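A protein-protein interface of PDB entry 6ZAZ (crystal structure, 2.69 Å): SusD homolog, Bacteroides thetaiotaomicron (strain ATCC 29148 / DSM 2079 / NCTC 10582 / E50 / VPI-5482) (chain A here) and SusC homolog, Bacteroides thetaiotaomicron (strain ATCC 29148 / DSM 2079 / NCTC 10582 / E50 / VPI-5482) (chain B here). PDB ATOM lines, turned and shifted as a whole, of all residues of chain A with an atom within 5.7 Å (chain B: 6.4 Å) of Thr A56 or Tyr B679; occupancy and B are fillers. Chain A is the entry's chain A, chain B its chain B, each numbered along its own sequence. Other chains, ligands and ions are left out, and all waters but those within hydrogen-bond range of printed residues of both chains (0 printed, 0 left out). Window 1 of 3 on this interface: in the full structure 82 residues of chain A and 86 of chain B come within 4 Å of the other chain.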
ATOM      1  N   ALA A  52     -17.610  -0.643 -17.053  1.00  0.00           N
ATOM      2  CA  ALA A  52     -16.339   0.033 -16.787  1.00  0.00           C
ATOM      3  C   ALA A  52     -16.191   1.373 -17.519  1.00  0.00           C
ATOM      4  O   ALA A  52     -15.686   2.347 -16.942  1.00  0.00           O
ATOM      5  CB  ALA A  52     -15.186  -0.895 -17.166  1.00  0.00           C
ATOM      6  N   ILE A  53     -16.607   1.443 -18.790  1.00  0.00           N
ATOM      7  CA  ILE A  53     -16.339   2.650 -19.564  1.00  0.00           C
ATOM      8  C   ILE A  53     -17.073   3.864 -18.998  1.00  0.00           C
ATOM      9  O   ILE A  53     -16.609   4.994 -19.189  1.00  0.00           O
ATOM     10  CB  ILE A  53     -16.652   2.437 -21.067  1.00  0.00           C
ATOM     11  CG1 ILE A  53     -16.090   3.574 -21.904  1.00  0.00           C
ATOM     12  CG2 ILE A  53     -18.136   2.254 -21.361  1.00  0.00           C
ATOM     13  CD1 ILE A  53     -15.800   3.146 -23.300  1.00  0.00           C
ATOM     14  N   TRP A  54     -18.180   3.675 -18.273  1.00  0.00           N
ATOM     15  CA  TRP A  54     -18.819   4.810 -17.603  1.00  0.00           C
ATOM     16  C   TRP A  54     -17.962   5.337 -16.467  1.00  0.00           C
ATOM     17  O   TRP A  54     -18.137   6.489 -16.055  1.00  0.00           O
ATOM     18  CB  TRP A  54     -20.219   4.428 -17.092  1.00  0.00           C
ATOM     19  CG  TRP A  54     -21.098   4.073 -18.234  1.00  0.00           C
ATOM     20  CD1 TRP A  54     -21.413   2.820 -18.670  1.00  0.00           C
ATOM     21  CD2 TRP A  54     -21.711   4.982 -19.149  1.00  0.00           C
ATOM     22  NE1 TRP A  54     -22.205   2.887 -19.786  1.00  0.00           N
ATOM     23  CE2 TRP A  54     -22.409   4.204 -20.104  1.00  0.00           C
ATOM     24  CE3 TRP A  54     -21.757   6.379 -19.245  1.00  0.00           C
ATOM     25  CZ2 TRP A  54     -23.148   4.776 -21.148  1.00  0.00           C
ATOM     26  CZ3 TRP A  54     -22.478   6.945 -20.283  1.00  0.00           C
ATOM     27  CH2 TRP A  54     -23.169   6.143 -21.223  1.00  0.00           C
ATOM     28  N   ALA A  55     -17.028   4.524 -15.964  1.00  0.00           N
ATOM     29  CA  ALA A  55     -16.047   5.000 -15.001  1.00  0.00           C
ATOM     30  C   ALA A  55     -14.748   5.412 -15.656  1.00  0.00           C
ATOM     31  O   ALA A  55     -14.102   6.345 -15.168  1.00  0.00           O
ATOM     32  CB  ALA A  55     -15.758   3.928 -13.952  1.00  0.00           C
ATOM     33  N   THR A  56     -14.353   4.762 -16.756  1.00  0.00           N
ATOM     34  CA  THR A  56     -13.012   4.946 -17.303  1.00  0.00           C
ATOM     35  C   THR A  56     -12.952   5.655 -18.655  1.00  0.00           C
ATOM     36  O   THR A  56     -11.872   5.702 -19.263  1.00  0.00           O
ATOM     37  CB  THR A  56     -12.335   3.597 -17.432  1.00  0.00           C
ATOM     38  OG1 THR A  56     -13.086   2.808 -18.354  1.00  0.00           O
ATOM     39  CG2 THR A  56     -12.277   2.909 -16.072  1.00  0.00           C
ATOM     40  N   GLY A  57     -14.065   6.199 -19.143  1.00  0.00           N
ATOM     41  CA  GLY A  57     -14.135   6.701 -20.499  1.00  0.00           C
ATOM     42  C   GLY A  57     -14.248   8.208 -20.570  1.00  0.00           C
ATOM     43  O   GLY A  57     -14.011   8.802 -21.629  1.00  0.00           O
ATOM     44  N   ASP A  58     -14.608   8.840 -19.459  1.00  0.00           N
ATOM     45  CA  ASP A  58     -14.637  10.292 -19.399  1.00  0.00           C
ATOM     46  C   ASP A  58     -13.312  10.805 -18.851  1.00  0.00           C
ATOM     47  O   ASP A  58     -12.483  10.046 -18.350  1.00  0.00           O
ATOM     48  CB  ASP A  58     -15.825  10.799 -18.563  1.00  0.00           C
ATOM     49  CG  ASP A  58     -15.844  10.247 -17.157  1.00  0.00           C
ATOM     50  OD1 ASP A  58     -15.000   9.382 -16.857  1.00  0.00           O
ATOM     51  OD2 ASP A  58     -16.709  10.670 -16.353  1.00  0.00           O
ATOM     52  N   PHE A  64     -19.083  12.139 -17.683  1.00  0.00           N
ATOM     53  CA  PHE A  64     -20.399  11.612 -18.031  1.00  0.00           C
ATOM     54  C   PHE A  64     -21.484  12.042 -17.046  1.00  0.00           C
ATOM     55  O   PHE A  64     -22.626  11.596 -17.159  1.00  0.00           O
ATOM     56  CB  PHE A  64     -20.348  10.088 -18.132  1.00  0.00           C
ATOM     57  CG  PHE A  64     -19.443   9.590 -19.221  1.00  0.00           C
ATOM     58  CD1 PHE A  64     -19.313  10.304 -20.421  1.00  0.00           C
ATOM     59  CD2 PHE A  64     -18.700   8.421 -19.042  1.00  0.00           C
ATOM     60  CE1 PHE A  64     -18.463   9.860 -21.428  1.00  0.00           C
ATOM     61  CE2 PHE A  64     -17.840   7.964 -20.029  1.00  0.00           C
ATOM     62  CZ  PHE A  64     -17.722   8.679 -21.230  1.00  0.00           C
ATOM     63  N   ARG A 111     -17.008  10.223 -27.332  1.00  0.00           N
ATOM     64  CA  ARG A 111     -16.963   9.421 -26.105  1.00  0.00           C
ATOM     65  C   ARG A 111     -18.273   8.685 -25.834  1.00  0.00           C
ATOM     66  O   ARG A 111     -18.263   7.504 -25.481  1.00  0.00           O
ATOM     67  CB  ARG A 111     -16.608  10.307 -24.908  1.00  0.00           C
ATOM     68  CG  ARG A 111     -15.165  10.809 -24.930  1.00  0.00           C
ATOM     69  CD  ARG A 111     -14.737  11.394 -23.606  1.00  0.00           C
ATOM     70  NE  ARG A 111     -13.499  12.149 -23.740  1.00  0.00           N
ATOM     71  CZ  ARG A 111     -12.323  11.742 -23.289  1.00  0.00           C
ATOM     72  NH1 ARG A 111     -12.213  10.571 -22.670  1.00  0.00           N
ATOM     73  NH2 ARG A 111     -11.252  12.498 -23.471  1.00  0.00           N
ATOM     74  N   GLN A 114     -18.726   5.763 -27.769  1.00  0.00           N
ATOM     75  CA  GLN A 114     -17.799   4.723 -27.345  1.00  0.00           C
ATOM     76  C   GLN A 114     -18.415   3.842 -26.265  1.00  0.00           C
ATOM     77  O   GLN A 114     -18.353   2.607 -26.343  1.00  0.00           O
ATOM     78  CB  GLN A 114     -16.508   5.350 -26.850  1.00  0.00           C
ATOM     79  CG  GLN A 114     -15.515   5.570 -27.936  1.00  0.00           C
ATOM     80  CD  GLN A 114     -14.362   6.384 -27.458  1.00  0.00           C
ATOM     81  OE1 GLN A 114     -14.558   7.370 -26.756  1.00  0.00           O
ATOM     82  NE2 GLN A 114     -13.149   5.989 -27.831  1.00  0.00           N
ATOM     83  N   ARG A 118     -19.409  -0.696 -26.308  1.00  0.00           N
ATOM     84  CA  ARG A 118     -19.240  -1.783 -25.358  1.00  0.00           C
ATOM     85  C   ARG A 118     -20.573  -2.443 -25.045  1.00  0.00           C
ATOM     86  O   ARG A 118     -20.642  -3.666 -24.896  1.00  0.00           O
ATOM     87  CB  ARG A 118     -18.555  -1.262 -24.091  1.00  0.00           C
ATOM     88  CG  ARG A 118     -17.115  -0.849 -24.321  1.00  0.00           C
ATOM     89  CD  ARG A 118     -16.304  -0.945 -23.071  1.00  0.00           C
ATOM     90  NE  ARG A 118     -14.950  -0.411 -23.226  1.00  0.00           N
ATOM     91  CZ  ARG A 118     -14.181  -0.037 -22.200  1.00  0.00           C
ATOM     92  NH1 ARG A 118     -14.639  -0.135 -20.957  1.00  0.00           N
ATOM     93  NH2 ARG A 118     -12.960   0.433 -22.406  1.00  0.00           N
ATOM     94  N   ASN A 301     -10.345   3.566  -9.523  1.00  0.00           N
ATOM     95  CA  ASN A 301     -11.429   3.937 -10.438  1.00  0.00           C
ATOM     96  C   ASN A 301     -12.195   5.114  -9.836  1.00  0.00           C
ATOM     97  O   ASN A 301     -13.390   5.066  -9.535  1.00  0.00           O
ATOM     98  CB  ASN A 301     -12.343   2.750 -10.721  1.00  0.00           C
ATOM     99  CG  ASN A 301     -11.993   2.004 -12.025  1.00  0.00           C
ATOM    100  OD1 ASN A 301     -10.955   2.246 -12.666  1.00  0.00           O
ATOM    101  ND2 ASN A 301     -12.877   1.070 -12.408  1.00  0.00           N
ATOM    102  N   PRO B 666      -7.371  -6.998 -22.597  1.00  0.00           N
ATOM    103  CA  PRO B 666      -7.996  -6.978 -21.267  1.00  0.00           C
ATOM    104  C   PRO B 666      -7.939  -5.608 -20.590  1.00  0.00           C
ATOM    105  O   PRO B 666      -8.897  -5.249 -19.893  1.00  0.00           O
ATOM    106  CB  PRO B 666      -7.224  -8.059 -20.489  1.00  0.00           C
ATOM    107  CG  PRO B 666      -6.042  -8.411 -21.325  1.00  0.00           C
ATOM    108  CD  PRO B 666      -6.382  -8.080 -22.738  1.00  0.00           C
ATOM    109  N   ASN B 667      -6.862  -4.842 -20.783  1.00  0.00           N
ATOM    110  CA  ASN B 667      -6.682  -3.487 -20.251  1.00  0.00           C
ATOM    111  C   ASN B 667      -7.461  -3.228 -18.965  1.00  0.00           C
ATOM    112  O   ASN B 667      -8.356  -2.376 -18.929  1.00  0.00           O
ATOM    113  CB  ASN B 667      -7.064  -2.475 -21.321  1.00  0.00           C
ATOM    114  CG  ASN B 667      -6.712  -1.059 -20.953  1.00  0.00           C
ATOM    115  OD1 ASN B 667      -7.605  -0.215 -20.829  1.00  0.00           O
ATOM    116  ND2 ASN B 667      -5.415  -0.769 -20.821  1.00  0.00           N
ATOM    117  N   TYR B 668      -7.146  -4.001 -17.919  1.00  0.00           N
ATOM    118  CA  TYR B 668      -7.737  -3.801 -16.598  1.00  0.00           C
ATOM    119  C   TYR B 668      -7.649  -2.345 -16.177  1.00  0.00           C
ATOM    120  O   TYR B 668      -8.548  -1.831 -15.499  1.00  0.00           O
ATOM    121  CB  TYR B 668      -7.026  -4.712 -15.582  1.00  0.00           C
ATOM    122  CG  TYR B 668      -7.566  -4.682 -14.159  1.00  0.00           C
ATOM    123  CD1 TYR B 668      -7.225  -3.662 -13.268  1.00  0.00           C
ATOM    124  CD2 TYR B 668      -8.392  -5.695 -13.693  1.00  0.00           C
ATOM    125  CE1 TYR B 668      -7.724  -3.640 -11.952  1.00  0.00           C
ATOM    126  CE2 TYR B 668      -8.886  -5.687 -12.387  1.00  0.00           C
ATOM    127  CZ  TYR B 668      -8.546  -4.662 -11.519  1.00  0.00           C
ATOM    128  OH  TYR B 668      -9.042  -4.679 -10.224  1.00  0.00           O
ATOM    129  N   GLY B 669      -6.574  -1.669 -16.579  1.00  0.00           N
ATOM    130  CA  GLY B 669      -6.402  -0.257 -16.338  1.00  0.00           C
ATOM    131  C   GLY B 669      -5.345  -0.033 -15.291  1.00  0.00           C
ATOM    132  O   GLY B 669      -5.640   0.519 -14.229  1.00  0.00           O
ATOM    133  N   SER B 673      -2.745   7.421 -16.724  1.00  0.00           N
ATOM    134  CA  SER B 673      -3.531   8.138 -17.688  1.00  0.00           C
ATOM    135  C   SER B 673      -3.196   9.627 -17.562  1.00  0.00           C
ATOM    136  O   SER B 673      -2.053   9.976 -17.217  1.00  0.00           O
ATOM    137  CB  SER B 673      -5.002   7.804 -17.460  1.00  0.00           C
ATOM    138  OG  SER B 673      -5.808   8.363 -18.475  1.00  0.00           O
ATOM    139  N   GLY B 676      -7.996  10.981 -16.081  1.00  0.00           N
ATOM    140  CA  GLY B 676      -8.909   9.889 -16.374  1.00  0.00           C
ATOM    141  C   GLY B 676      -8.735   9.377 -17.795  1.00  0.00           C
ATOM    142  O   GLY B 676      -7.677   9.529 -18.405  1.00  0.00           O
ATOM    143  N   GLN B 677      -9.802   8.775 -18.331  1.00  0.00           N
ATOM    144  CA  GLN B 677      -9.793   8.167 -19.669  1.00  0.00           C
ATOM    145  C   GLN B 677      -8.661   7.130 -19.780  1.00  0.00           C
ATOM    146  O   GLN B 677      -7.887   7.079 -20.743  1.00  0.00           O
ATOM    147  CB  GLN B 677      -9.755   9.247 -20.775  1.00  0.00           C
ATOM    148  CG  GLN B 677      -8.408   9.648 -21.389  1.00  0.00           C
ATOM    149  CD  GLN B 677      -8.501  10.782 -22.393  1.00  0.00           C
ATOM    150  OE1 GLN B 677      -9.381  10.797 -23.261  1.00  0.00           O
ATOM    151  NE2 GLN B 677      -7.586  11.748 -22.278  1.00  0.00           N
ATOM    152  N   SER B 678      -8.567   6.280 -18.748  1.00  0.00           N
ATOM    153  CA  SER B 678      -7.765   5.062 -18.863  1.00  0.00           C
ATOM    154  C   SER B 678      -8.406   4.062 -19.819  1.00  0.00           C
ATOM    155  O   SER B 678      -7.698   3.243 -20.421  1.00  0.00           O
ATOM    156  CB  SER B 678      -7.604   4.413 -17.504  1.00  0.00           C
ATOM    157  OG  SER B 678      -8.769   3.664 -17.173  1.00  0.00           O
ATOM    158  N   TYR B 679      -9.745   4.117 -19.960  1.00  0.00           N
ATOM    159  CA  TYR B 679     -10.516   3.193 -20.789  1.00  0.00           C
ATOM    160  C   TYR B 679     -10.354   1.753 -20.317  1.00  0.00           C
ATOM    161  O   TYR B 679     -10.329   0.824 -21.132  1.00  0.00           O
ATOM    162  CB  TYR B 679     -10.138   3.316 -22.274  1.00  0.00           C
ATOM    163  CG  TYR B 679     -10.727   4.533 -22.977  1.00  0.00           C
ATOM    164  CD1 TYR B 679     -12.027   4.508 -23.491  1.00  0.00           C
ATOM    165  CD2 TYR B 679      -9.987   5.712 -23.117  1.00  0.00           C
ATOM    166  CE1 TYR B 679     -12.575   5.619 -24.124  1.00  0.00           C
ATOM    167  CE2 TYR B 679     -10.524   6.826 -23.743  1.00  0.00           C
ATOM    168  CZ  TYR B 679     -11.825   6.773 -24.253  1.00  0.00           C
ATOM    169  OH  TYR B 679     -12.376   7.868 -24.886  1.00  0.00           O
ATOM    170  N   GLY B 680     -10.224   1.569 -18.997  1.00  0.00           N
ATOM    171  CA  GLY B 680     -10.005   0.246 -18.447  1.00  0.00           C
ATOM    172  C   GLY B 680     -11.279  -0.569 -18.429  1.00  0.00           C
ATOM    173  O   GLY B 680     -12.383  -0.040 -18.528  1.00  0.00           O
ATOM    174  N   THR B 681     -11.134  -1.889 -18.308  1.00  0.00           N
ATOM    175  CA  THR B 681     -12.309  -2.752 -18.265  1.00  0.00           C
ATOM    176  C   THR B 681     -12.680  -3.219 -16.859  1.00  0.00           C
ATOM    177  O   THR B 681     -13.688  -3.908 -16.699  1.00  0.00           O
ATOM    178  CB  THR B 681     -12.118  -3.960 -19.186  1.00  0.00           C
ATOM    179  OG1 THR B 681     -11.272  -4.927 -18.562  1.00  0.00           O
ATOM    180  CG2 THR B 681     -11.486  -3.515 -20.500  1.00  0.00           C
ATOM    181  N   ALA B 682     -11.916  -2.857 -15.837  1.00  0.00           N
ATOM    182  CA  ALA B 682     -12.321  -3.187 -14.479  1.00  0.00           C
ATOM    183  C   ALA B 682     -13.472  -2.288 -14.036  1.00  0.00           C
ATOM    184  O   ALA B 682     -13.580  -1.129 -14.453  1.00  0.00           O
ATOM    185  CB  ALA B 682     -11.136  -3.042 -13.526  1.00  0.00           C
ATOM    186  N   LYS B 699     -11.639  -4.726 -24.286  1.00  0.00           N
ATOM    187  CA  LYS B 699     -12.041  -3.571 -25.071  1.00  0.00           C
ATOM    188  C   LYS B 699     -11.349  -3.623 -26.428  1.00  0.00           C
ATOM    189  O   LYS B 699     -10.179  -4.014 -26.530  1.00  0.00           O
ATOM    190  CB  LYS B 699     -11.737  -2.244 -24.353  1.00  0.00           C
ATOM    191  CG  LYS B 699     -10.280  -2.004 -24.063  1.00  0.00           C
ATOM    192  CD  LYS B 699      -9.677  -0.956 -24.974  1.00  0.00           C
ATOM    193  CE  LYS B 699      -8.380  -0.433 -24.386  1.00  0.00           C
ATOM    194  NZ  LYS B 699      -7.634   0.443 -25.332  1.00  0.00           N
ATOM    195  N   GLU B 755     -15.536   2.664 -29.965  1.00  0.00           N
ATOM    196  CA  GLU B 755     -14.260   2.324 -29.328  1.00  0.00           C
ATOM    197  C   GLU B 755     -13.397   1.455 -30.229  1.00  0.00           C
ATOM    198  O   GLU B 755     -13.816   0.387 -30.669  1.00  0.00           O
ATOM    199  CB  GLU B 755     -14.497   1.627 -27.995  1.00  0.00           C
ATOM    200  CG  GLU B 755     -13.322   1.769 -27.091  1.00  0.00           C
ATOM    201  CD  GLU B 755     -13.397   0.928 -25.834  1.00  0.00           C
ATOM    202  OE1 GLU B 755     -14.344   0.115 -25.665  1.00  0.00           O
ATOM    203  OE2 GLU B 755     -12.460   1.079 -25.015  1.00  0.00           O
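The side-chain amide nitrogen (ND2) of Asn A301 sits at hydrogen-bond distance from the backbone carbonyl oxygen (O) of Ala B682.
The side-chain hydroxyl (OG1) of Thr A56 lies within hydrogen-bond range of the backbone carbonyl oxygen (O) of Gly B680, 2.9 Å away.
The side-chain amide oxygen (OE1) of Gln B677 sits at hydrogen-bond distance from the guanidinium group (NH2) of Arg A111, 2.5 Å away.
The guanidinium group (NH2) of Arg A118 lies within hydrogen-bond range of the backbone carbonyl oxygen (O) of Tyr B679, 2.9 Å away.
The side-chain hydroxyl of Tyr B679 is in hydrogen-bond range of the guanidinium group of Arg A111, at 3.5 Å.
N of Ser B678 lies within hydrogen-bond range of O of Thr A56, at 3.4 Å.
O of Thr A56 sits at hydrogen-bond distance from N of Tyr B679, 2.7 Å away.
OH of Tyr B679 sits at hydrogen-bond distance from OE1 of Gln A114.
O of Gly B680 is in hydrogen-bond range of NH1 of Arg A118, 3.3 Å away.
O of Asp A58 lies within hydrogen-bond range of N of Gln B677 (3.0 Å).
The guanidinium group (NE) of Arg A118 is in salt-bridge range of the side-chain carboxylate (OE1) of Glu B755.
NH1 of Arg A111 lies within hydrogen-bond range of O of Gly A57, at 2.7 Å.
The backbone carbonyl oxygen (O) of Tyr B679 lies close to the side-chain amide oxygen (OD1) of Asn B667 (2.9 Å).
OD2 of Asp A58 lies within hydrogen-bond range of N of Phe A64 (3.1 Å).
The side-chain hydroxyl (OG) of Ser B678 sits at hydrogen-bond distance from the backbone NH (N) of Gly B680 (3.1 Å).
O of Pro B666 is in hydrogen-bond range of OG1 of Thr B681.
O of Asn B667 lies within hydrogen-bond range of N of Thr B681.
CB of Ala A52 touches O of Gly B680, at 3.2 Å.
Ala A52 touches Thr B681.
O of Ala B682 touches CB of Ala A52, at 3.2 Å.
O of Thr A56 touches CA of Gln B677 (3.3 Å).
O of Gly A57 touches OH of Tyr B679, 3.8 Å away.
Asp A58 touches Gly B676 (O to C, 3.8 Å).
Glu B755 touches Gln A114.
CB of Lys B699 touches NH2 of Arg A118, at 3.5 Å.
Trp A54 touches none of the printed residues of chain B.
Phe A64 touches none of the printed residues of chain B.
Of the printed residues of chain B, Arg A111 touches Gln B677 and Tyr B679.
Printed residues of chain B within 4 Å of Gln A114: Tyr B679 (2.9 Å) and Glu B755 (3.5 Å).
Printed residues of chain A within 4 Å of Tyr B679: Thr A56, Gly A57, Arg A111, Gln A114 and Arg A118.
Of the printed residues of chain A, Thr B681 touches Ala A52 (3.4 Å).
Printed residues of chain A within 4 Å of Ala B682: Ala A52 and Asn A301.
Of the printed residues of chain A, Glu B755 touches Gln A114 and Arg A118.
The nearest printed residue of chain A that does not touch Tyr B679 is Ile A53 (4.02 Å).
The nearest printed residue of chain A that does not touch Ala B682 is Thr A56 (4.5 Å).
Printed residues of chain B that touch a printed residue of chain A: Gly B676, Gln B677, Ser B678, Tyr B679, Gly B680, Thr B681, Ala B682, Lys B699 and Glu B755.
Hydrophobic or aromatic side chains of chain B that line the printed part of chain A: Tyr B679.
Printed residues of chain A that touch a printed residue of chain B: Ala A52, Thr A56, Gly A57, Asp A58, Arg A111, Gln A114, Arg A118 and Asn A301.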
